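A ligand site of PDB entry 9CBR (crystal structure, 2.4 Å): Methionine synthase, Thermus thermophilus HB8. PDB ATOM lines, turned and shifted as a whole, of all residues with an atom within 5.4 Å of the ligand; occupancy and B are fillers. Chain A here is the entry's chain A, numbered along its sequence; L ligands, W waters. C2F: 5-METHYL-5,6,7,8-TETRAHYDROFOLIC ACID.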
ATOM      1  N   GLU A 373      23.143 -26.805  -6.984  1.00  0.00           N
ATOM      2  CA  GLU A 373      23.317 -26.026  -8.196  1.00  0.00           C
ATOM      3  C   GLU A 373      22.034 -25.883  -9.008  1.00  0.00           C
ATOM      4  O   GLU A 373      22.008 -25.056  -9.932  1.00  0.00           O
ATOM      5  CB  GLU A 373      24.350 -26.642  -9.139  1.00  0.00           C
ATOM      6  CG  GLU A 373      23.968 -28.059  -9.593  1.00  0.00           C
ATOM      7  CD  GLU A 373      24.778 -28.687 -10.658  1.00  0.00           C
ATOM      8  OE1 GLU A 373      26.017 -28.509 -10.712  1.00  0.00           O
ATOM      9  OE2 GLU A 373      24.040 -29.421 -11.400  1.00  0.00           O
ATOM     10  N   ARG A 374      20.961 -26.568  -8.585  1.00  0.00           N
ATOM     11  CA  ARG A 374      19.804 -26.823  -9.415  1.00  0.00           C
ATOM     12  C   ARG A 374      18.774 -25.712  -9.505  1.00  0.00           C
ATOM     13  O   ARG A 374      17.952 -25.810 -10.400  1.00  0.00           O
ATOM     14  CB  ARG A 374      19.093 -28.128  -9.022  1.00  0.00           C
ATOM     15  CG  ARG A 374      19.964 -29.362  -9.117  1.00  0.00           C
ATOM     16  CD  ARG A 374      19.179 -30.593  -8.798  1.00  0.00           C
ATOM     17  NE  ARG A 374      18.317 -31.023  -9.906  1.00  0.00           N
ATOM     18  CZ  ARG A 374      17.280 -31.844  -9.856  1.00  0.00           C
ATOM     19  NH1 ARG A 374      17.013 -32.502  -8.746  1.00  0.00           N
ATOM     20  NH2 ARG A 374      16.521 -31.999 -10.943  1.00  0.00           N
ATOM     21  N   ASN A 376      19.072 -22.989 -11.163  1.00  0.00           N
ATOM     22  CA  ASN A 376      19.783 -22.244 -12.188  1.00  0.00           C
ATOM     23  C   ASN A 376      18.963 -22.350 -13.480  1.00  0.00           C
ATOM     24  O   ASN A 376      18.764 -23.437 -13.932  1.00  0.00           O
ATOM     25  CB  ASN A 376      21.229 -22.708 -12.172  1.00  0.00           C
ATOM     26  CG  ASN A 376      22.088 -22.109 -13.255  1.00  0.00           C
ATOM     27  OD1 ASN A 376      21.619 -21.846 -14.384  1.00  0.00           O
ATOM     28  ND2 ASN A 376      23.388 -22.004 -12.932  1.00  0.00           N
ATOM     29  N   THR A 378      19.403 -21.561 -16.608  1.00  0.00           N
ATOM     30  CA  THR A 378      20.136 -22.172 -17.727  1.00  0.00           C
ATOM     31  C   THR A 378      20.401 -23.665 -17.487  1.00  0.00           C
ATOM     32  O   THR A 378      20.177 -24.448 -18.421  1.00  0.00           O
ATOM     33  CB  THR A 378      21.399 -21.361 -17.999  1.00  0.00           C
ATOM     34  OG1 THR A 378      21.972 -20.917 -16.786  1.00  0.00           O
ATOM     35  CG2 THR A 378      21.135 -20.083 -18.761  1.00  0.00           C
ATOM     36  N   GLY A 379      20.783 -24.041 -16.239  1.00  0.00           N
ATOM     37  CA  GLY A 379      21.270 -25.364 -15.884  1.00  0.00           C
ATOM     38  C   GLY A 379      20.255 -26.304 -15.222  1.00  0.00           C
ATOM     39  O   GLY A 379      20.678 -27.284 -14.544  1.00  0.00           O
ATOM     40  N   SER A 380      18.962 -26.073 -15.395  1.00  0.00           N
ATOM     41  CA  SER A 380      17.955 -27.020 -14.903  1.00  0.00           C
ATOM     42  C   SER A 380      16.610 -26.755 -15.575  1.00  0.00           C
ATOM     43  O   SER A 380      15.974 -25.712 -15.254  1.00  0.00           O
ATOM     44  CB  SER A 380      17.754 -26.969 -13.384  1.00  0.00           C
ATOM     45  OG  SER A 380      16.578 -27.714 -13.010  1.00  0.00           O
ATOM     46  N   LYS A 381      16.222 -27.664 -16.494  1.00  0.00           N
ATOM     47  CA  LYS A 381      14.970 -27.616 -17.209  1.00  0.00           C
ATOM     48  C   LYS A 381      13.790 -27.478 -16.250  1.00  0.00           C
ATOM     49  O   LYS A 381      12.908 -26.667 -16.520  1.00  0.00           O
ATOM     50  CB  LYS A 381      14.761 -28.909 -18.021  1.00  0.00           C
ATOM     51  CG  LYS A 381      13.586 -28.881 -19.023  1.00  0.00           C
ATOM     52  CD  LYS A 381      13.649 -30.024 -20.019  1.00  0.00           C
ATOM     53  CE  LYS A 381      12.620 -29.956 -21.070  1.00  0.00           C
ATOM     54  NZ  LYS A 381      11.276 -30.099 -20.526  1.00  0.00           N
ATOM     55  N   ARG A 382      13.803 -28.242 -15.141  1.00  0.00           N
ATOM     56  CA  ARG A 382      12.697 -28.314 -14.182  1.00  0.00           C
ATOM     57  C   ARG A 382      12.510 -26.969 -13.487  1.00  0.00           C
ATOM     58  O   ARG A 382      11.356 -26.545 -13.276  1.00  0.00           O
ATOM     59  CB  ARG A 382      13.002 -29.498 -13.251  1.00  0.00           C
ATOM     60  CG  ARG A 382      11.886 -29.877 -12.280  1.00  0.00           C
ATOM     61  CD  ARG A 382      11.758 -31.357 -11.893  1.00  0.00           C
ATOM     62  NE  ARG A 382      12.886 -31.952 -11.165  1.00  0.00           N
ATOM     63  CZ  ARG A 382      12.958 -32.100  -9.843  1.00  0.00           C
ATOM     64  NH1 ARG A 382      11.987 -31.644  -9.093  1.00  0.00           N
ATOM     65  NH2 ARG A 382      14.007 -32.700  -9.283  1.00  0.00           N
ATOM     66  N   ASP A 411      22.601 -22.208  -4.702  1.00  0.00           N
ATOM     67  CA  ASP A 411      22.914 -21.212  -5.733  1.00  0.00           C
ATOM     68  C   ASP A 411      21.646 -20.797  -6.468  1.00  0.00           C
ATOM     69  O   ASP A 411      20.894 -21.660  -6.925  1.00  0.00           O
ATOM     70  CB  ASP A 411      23.846 -21.898  -6.728  1.00  0.00           C
ATOM     71  CG  ASP A 411      24.605 -21.009  -7.685  1.00  0.00           C
ATOM     72  OD1 ASP A 411      25.389 -20.208  -7.177  1.00  0.00           O
ATOM     73  OD2 ASP A 411      24.348 -21.124  -8.916  1.00  0.00           O
ATOM     74  N   ASP A 443      23.661 -15.673  -7.703  1.00  0.00           N
ATOM     75  CA  ASP A 443      24.419 -15.933  -8.918  1.00  0.00           C
ATOM     76  C   ASP A 443      23.926 -14.961  -9.987  1.00  0.00           C
ATOM     77  O   ASP A 443      22.788 -15.087 -10.477  1.00  0.00           O
ATOM     78  CB  ASP A 443      24.287 -17.391  -9.359  1.00  0.00           C
ATOM     79  CG  ASP A 443      25.364 -17.967 -10.277  1.00  0.00           C
ATOM     80  OD1 ASP A 443      26.313 -17.217 -10.680  1.00  0.00           O
ATOM     81  OD2 ASP A 443      25.275 -19.210 -10.565  1.00  0.00           O
ATOM     82  N   ASN A 464      28.082 -14.302  -5.933  1.00  0.00           N
ATOM     83  CA  ASN A 464      28.769 -15.058  -6.957  1.00  0.00           C
ATOM     84  C   ASN A 464      28.492 -14.351  -8.270  1.00  0.00           C
ATOM     85  O   ASN A 464      27.323 -14.364  -8.690  1.00  0.00           O
ATOM     86  CB  ASN A 464      28.343 -16.528  -6.922  1.00  0.00           C
ATOM     87  CG  ASN A 464      28.825 -17.404  -8.046  1.00  0.00           C
ATOM     88  OD1 ASN A 464      29.810 -17.115  -8.733  1.00  0.00           O
ATOM     89  ND2 ASN A 464      28.170 -18.521  -8.215  1.00  0.00           N
ATOM     90  N   VAL A 490      32.544 -14.619  -3.747  1.00  0.00           N
ATOM     91  CA  VAL A 490      33.208 -15.543  -4.657  1.00  0.00           C
ATOM     92  C   VAL A 490      34.004 -14.636  -5.591  1.00  0.00           C
ATOM     93  O   VAL A 490      33.456 -13.671  -6.113  1.00  0.00           O
ATOM     94  CB  VAL A 490      32.235 -16.459  -5.435  1.00  0.00           C
ATOM     95  CG1 VAL A 490      32.936 -17.228  -6.522  1.00  0.00           C
ATOM     96  CG2 VAL A 490      31.499 -17.429  -4.550  1.00  0.00           C
ATOM     97  N   LEU A 492      36.085 -14.817  -8.992  1.00  0.00           N
ATOM     98  CA  LEU A 492      36.388 -15.586 -10.197  1.00  0.00           C
ATOM     99  C   LEU A 492      37.670 -15.074 -10.863  1.00  0.00           C
ATOM    100  O   LEU A 492      37.996 -13.920 -10.688  1.00  0.00           O
ATOM    101  CB  LEU A 492      35.133 -15.449 -11.054  1.00  0.00           C
ATOM    102  CG  LEU A 492      34.974 -16.348 -12.270  1.00  0.00           C
ATOM    103  CD1 LEU A 492      35.072 -17.783 -12.040  1.00  0.00           C
ATOM    104  CD2 LEU A 492      33.675 -16.073 -12.959  1.00  0.00           C
ATOM    105  N   ASP A 531      37.323 -18.820  -6.912  1.00  0.00           N
ATOM    106  CA  ASP A 531      36.953 -19.666  -8.022  1.00  0.00           C
ATOM    107  C   ASP A 531      38.011 -19.569  -9.132  1.00  0.00           C
ATOM    108  O   ASP A 531      37.944 -18.663  -9.978  1.00  0.00           O
ATOM    109  CB  ASP A 531      35.547 -19.352  -8.472  1.00  0.00           C
ATOM    110  CG  ASP A 531      34.872 -20.304  -9.463  1.00  0.00           C
ATOM    111  OD1 ASP A 531      35.360 -21.398  -9.650  1.00  0.00           O
ATOM    112  OD2 ASP A 531      33.847 -19.925 -10.082  1.00  0.00           O
ATOM    113  N   THR A 534      36.694 -24.136 -13.903  1.00  0.00           N
ATOM    114  CA  THR A 534      36.414 -25.495 -14.340  1.00  0.00           C
ATOM    115  C   THR A 534      35.980 -25.461 -15.809  1.00  0.00           C
ATOM    116  O   THR A 534      34.792 -25.251 -16.094  1.00  0.00           O
ATOM    117  CB  THR A 534      35.310 -26.142 -13.489  1.00  0.00           C
ATOM    118  OG1 THR A 534      35.720 -26.086 -12.134  1.00  0.00           O
ATOM    119  CG2 THR A 534      35.125 -27.628 -13.729  1.00  0.00           C
ATOM    120  N   VAL A 568      36.388 -22.277  -4.322  1.00  0.00           N
ATOM    121  CA  VAL A 568      35.115 -22.793  -4.803  1.00  0.00           C
ATOM    122  C   VAL A 568      35.289 -23.162  -6.273  1.00  0.00           C
ATOM    123  O   VAL A 568      36.162 -22.582  -6.927  1.00  0.00           O
ATOM    124  CB  VAL A 568      33.916 -21.846  -4.544  1.00  0.00           C
ATOM    125  CG1 VAL A 568      33.957 -20.562  -5.358  1.00  0.00           C
ATOM    126  CG2 VAL A 568      32.583 -22.539  -4.777  1.00  0.00           C
ATOM    127  N   LEU A 569      34.570 -24.216  -6.743  1.00  0.00           N
ATOM    128  CA  LEU A 569      34.545 -24.647  -8.137  1.00  0.00           C
ATOM    129  C   LEU A 569      33.142 -25.116  -8.501  1.00  0.00           C
ATOM    130  O   LEU A 569      32.447 -25.628  -7.639  1.00  0.00           O
ATOM    131  CB  LEU A 569      35.508 -25.793  -8.413  1.00  0.00           C
ATOM    132  CG  LEU A 569      37.007 -25.500  -8.522  1.00  0.00           C
ATOM    133  CD1 LEU A 569      37.698 -26.760  -8.903  1.00  0.00           C
ATOM    134  CD2 LEU A 569      37.397 -24.443  -9.515  1.00  0.00           C
ATOM    135  N   GLY A 570      32.734 -24.914  -9.767  1.00  0.00           N
ATOM    136  CA  GLY A 570      31.577 -25.599 -10.353  1.00  0.00           C
ATOM    137  C   GLY A 570      32.006 -26.892 -11.067  1.00  0.00           C
ATOM    138  O   GLY A 570      32.142 -26.930 -12.272  1.00  0.00           O
ATOM    139  N   SER A 572      30.617 -29.690 -12.016  1.00  0.00           N
ATOM    140  CA  SER A 572      29.797 -30.296 -13.070  1.00  0.00           C
ATOM    141  C   SER A 572      30.140 -29.807 -14.491  1.00  0.00           C
ATOM    142  O   SER A 572      29.638 -30.408 -15.439  1.00  0.00           O
ATOM    143  CB  SER A 572      28.282 -30.146 -12.756  1.00  0.00           C
ATOM    144  OG  SER A 572      27.975 -30.606 -11.431  1.00  0.00           O
ATOM    145  N   ASN A 573      30.986 -28.752 -14.675  1.00  0.00           N
ATOM    146  CA  ASN A 573      31.464 -28.283 -15.967  1.00  0.00           C
ATOM    147  C   ASN A 573      32.681 -29.053 -16.534  1.00  0.00           C
ATOM    148  O   ASN A 573      32.931 -28.936 -17.726  1.00  0.00           O
ATOM    149  CB  ASN A 573      31.835 -26.811 -15.914  1.00  0.00           C
ATOM    150  CG  ASN A 573      30.686 -25.894 -15.561  1.00  0.00           C
ATOM    151  OD1 ASN A 573      29.968 -25.412 -16.443  1.00  0.00           O
ATOM    152  ND2 ASN A 573      30.542 -25.540 -14.293  1.00  0.00           N
ATOM    153  N   PHE A 576      31.470 -31.919 -19.568  1.00  0.00           N
ATOM    154  CA  PHE A 576      30.572 -31.600 -20.690  1.00  0.00           C
ATOM    155  C   PHE A 576      31.036 -32.315 -21.958  1.00  0.00           C
ATOM    156  O   PHE A 576      32.246 -32.389 -22.211  1.00  0.00           O
ATOM    157  CB  PHE A 576      30.415 -30.132 -21.067  1.00  0.00           C
ATOM    158  CG  PHE A 576      29.396 -29.276 -20.317  1.00  0.00           C
ATOM    159  CD1 PHE A 576      28.047 -29.608 -20.233  1.00  0.00           C
ATOM    160  CD2 PHE A 576      29.812 -28.098 -19.689  1.00  0.00           C
ATOM    161  CE1 PHE A 576      27.163 -28.774 -19.541  1.00  0.00           C
ATOM    162  CE2 PHE A 576      28.938 -27.281 -19.006  1.00  0.00           C
ATOM    163  CZ  PHE A 576      27.607 -27.603 -18.958  1.00  0.00           C
ATOM    164  N   ARG A 583      29.240 -38.670 -16.769  1.00  0.00           N
ATOM    165  CA  ARG A 583      29.419 -37.341 -16.178  1.00  0.00           C
ATOM    166  C   ARG A 583      29.480 -37.409 -14.657  1.00  0.00           C
ATOM    167  O   ARG A 583      30.377 -36.841 -14.049  1.00  0.00           O
ATOM    168  CB  ARG A 583      28.328 -36.335 -16.563  1.00  0.00           C
ATOM    169  CG  ARG A 583      28.446 -35.833 -18.002  1.00  0.00           C
ATOM    170  CD  ARG A 583      27.576 -34.622 -18.286  1.00  0.00           C
ATOM    171  NE  ARG A 583      28.101 -33.341 -17.810  1.00  0.00           N
ATOM    172  CZ  ARG A 583      27.387 -32.226 -17.672  1.00  0.00           C
ATOM    173  NH1 ARG A 583      26.119 -32.198 -18.011  1.00  0.00           N
ATOM    174  NH2 ARG A 583      27.899 -31.134 -17.156  1.00  0.00           N
ATOM    175  N   ILE A 603      30.073 -26.100  -6.005  1.00  0.00           N
ATOM    176  CA  ILE A 603      28.775 -26.049  -6.634  1.00  0.00           C
ATOM    177  C   ILE A 603      28.575 -27.389  -7.384  1.00  0.00           C
ATOM    178  O   ILE A 603      29.349 -27.729  -8.294  1.00  0.00           O
ATOM    179  CB  ILE A 603      28.735 -24.810  -7.548  1.00  0.00           C
ATOM    180  CG1 ILE A 603      28.770 -23.472  -6.777  1.00  0.00           C
ATOM    181  CG2 ILE A 603      27.547 -24.832  -8.522  1.00  0.00           C
ATOM    182  CD1 ILE A 603      29.681 -22.431  -7.429  1.00  0.00           C
HETATM  183  N1  C2F L   1      29.368 -20.426 -10.381  1.00  0.00           N
HETATM  184  C2  C2F L   1      30.668 -20.422 -10.113  1.00  0.00           C
HETATM  185  NA2 C2F L   1      31.120 -19.752  -9.054  1.00  0.00           N
HETATM  186  N3  C2F L   1      31.564 -21.097 -10.927  1.00  0.00           N
HETATM  187  C4  C2F L   1      31.209 -21.824 -12.049  1.00  0.00           C
HETATM  188  O4  C2F L   1      32.089 -22.468 -12.674  1.00  0.00           O
HETATM  189  C4A C2F L   1      29.833 -21.871 -12.340  1.00  0.00           C
HETATM  190  N5  C2F L   1      29.294 -22.430 -13.461  1.00  0.00           N
HETATM  191  C6  C2F L   1      27.911 -22.925 -13.290  1.00  0.00           C
HETATM  192  C7  C2F L   1      27.029 -21.745 -12.917  1.00  0.00           C
HETATM  193  N8  C2F L   1      27.592 -21.004 -11.808  1.00  0.00           N
HETATM  194  C8A C2F L   1      28.944 -21.052 -11.518  1.00  0.00           C
HETATM  195  C9  C2F L   1      27.739 -24.038 -12.231  1.00  0.00           C
HETATM  196  N10 C2F L   1      26.379 -24.580 -12.266  1.00  0.00           N
HETATM  197  C11 C2F L   1      29.937 -22.386 -14.771  1.00  0.00           C
HETATM  198  C12 C2F L   1      25.017 -27.669 -14.720  1.00  0.00           C
HETATM  199  C13 C2F L   1      24.143 -27.031 -13.835  1.00  0.00           C
HETATM  200  C14 C2F L   1      24.571 -25.967 -13.051  1.00  0.00           C
HETATM  201  C15 C2F L   1      25.898 -25.548 -13.118  1.00  0.00           C
HETATM  202  C16 C2F L   1      26.767 -26.200 -13.993  1.00  0.00           C
HETATM  203  C17 C2F L   1      26.320 -27.232 -14.785  1.00  0.00           C
HETATM  204  C   C2F L   1      24.647 -28.792 -15.651  1.00  0.00           C
HETATM  205  O   C2F L   1      25.513 -29.554 -16.077  1.00  0.00           O
HETATM  206  N   C2F L   1      23.367 -28.863 -16.051  1.00  0.00           N
HETATM  207  CA  C2F L   1      22.863 -29.847 -17.007  1.00  0.00           C
HETATM  208  CB  C2F L   1      21.338 -29.940 -17.073  1.00  0.00           C
HETATM  209  CG  C2F L   1      20.656 -30.537 -15.851  1.00  0.00           C
HETATM  210  CD  C2F L   1      19.173 -30.811 -16.117  1.00  0.00           C
HETATM  211  OE1 C2F L   1      18.631 -31.772 -15.504  1.00  0.00           O
HETATM  212  OE2 C2F L   1      18.557 -30.031 -16.907  1.00  0.00           O
HETATM  213  CT  C2F L   1      23.338 -29.488 -18.432  1.00  0.00           C
HETATM  214  O1  C2F L   1      23.357 -30.430 -19.223  1.00  0.00           O
HETATM  215  O2  C2F L   1      23.727 -28.318 -18.685  1.00  0.00           O
HETATM  216  O   HOH W   1      17.336 -30.211 -12.828  1.00  0.00           O
HETATM  217  O   HOH W   2      24.357 -23.233 -10.713  1.00  0.00           O
HETATM  218  O   HOH W   3      34.371 -23.257 -11.227  1.00  0.00           O
HETATM  219  O   HOH W   4      20.614 -32.192 -20.305  1.00  0.00           O
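An oxygen (OE2) of the ligand is in hydrogen-bond range of the backbone NH of Lys 381 (3.4 Å). O of Gly 379 lies within hydrogen-bond range of N of the ligand (3.5 Å). An oxygen (O1) of the ligand lies within salt-bridge range of the guanidinium group (NH1) of Arg 583 (3.5 Å). N8 of the ligand is in hydrogen-bond range of OD2 of Asp 443 (3.2 Å). The side-chain carboxylate of Asp 531 sits at hydrogen-bond distance from a nitrogen (N3) of the ligand (2.7 Å). The side-chain amide oxygen of Asn 464 is in hydrogen-bond range of a nitrogen (NA2) of the ligand (3.0 Å).
The side-chain amide nitrogen of Asn 464 is in hydrogen-bond range of the side-chain carboxylate of Asp 411. The backbone carbonyl oxygen (O) of Ser 572 sits at hydrogen-bond distance from the guanidinium group (NH2) of Arg 583 (2.5 Å). The side-chain amide oxygen of Asn 376 sits at hydrogen-bond distance from the side-chain hydroxyl of Thr 378 (2.6 Å). OD2 of Asp 443 lies close to OD2 of Asp 411. ND2 of Asn 464 sits at hydrogen-bond distance from OD1 of Asp 443 (3.4 Å). ND2 of Asn 573 sits at hydrogen-bond distance from O of Gly 570 (2.9 Å). OG of Ser 572 sits at hydrogen-bond distance from OE1 of Glu 373 (3.0 Å). The backbone NH (N) of Ile 603 is in hydrogen-bond range of the backbone carbonyl oxygen (O) of Leu 569 (2.9 Å).
The side-chain amide nitrogen of Asn 573 sits close to a nitrogen (N5) of the ligand, 3.5 Å away. Glu 373 touches the ligand (OE2 to C13, 3.4 Å). ND2 of Asn 376 touches C7 of the ligand, at 3.7 Å. Ser 380 touches the ligand (CA to OE2, 3.7 Å). N of Gly 570 touches O4 of the ligand, 3.9 Å away. Phe 576 touches the ligand. Ile 603 touches the ligand (CD1 to NA2, 3.4 Å). Within 4 Å of the ligand: Glu 373, Asn 376, Gly 379, Ser 380, Lys 381, Asp 443, Asn 464, Asp 531, Gly 570, Asn 573, Phe 576, Arg 583 and Ile 603. The nearest printed residue that does not touch the ligand is Val 490 (4.01 Å).
Water W3 lies within hydrogen-bond range of OD1 of Asp 531, N of Gly 570, O4 of the ligand and OG1 of Thr 534. Water W2 lies within hydrogen-bond range of the side-chain amide nitrogen of Asn 376 (2.7 Å), the side-chain carboxylate of Asp 411 (2.8 Å), a nitrogen (N10) of the ligand (2.9 Å) and the backbone carbonyl oxygen of Glu 373 (3.1 Å). Water W1 lies within hydrogen-bond range of OG of Ser 380 (2.6 Å), NH2 of Arg 374 (2.7 Å) and OE1 of the ligand (3.4 Å).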
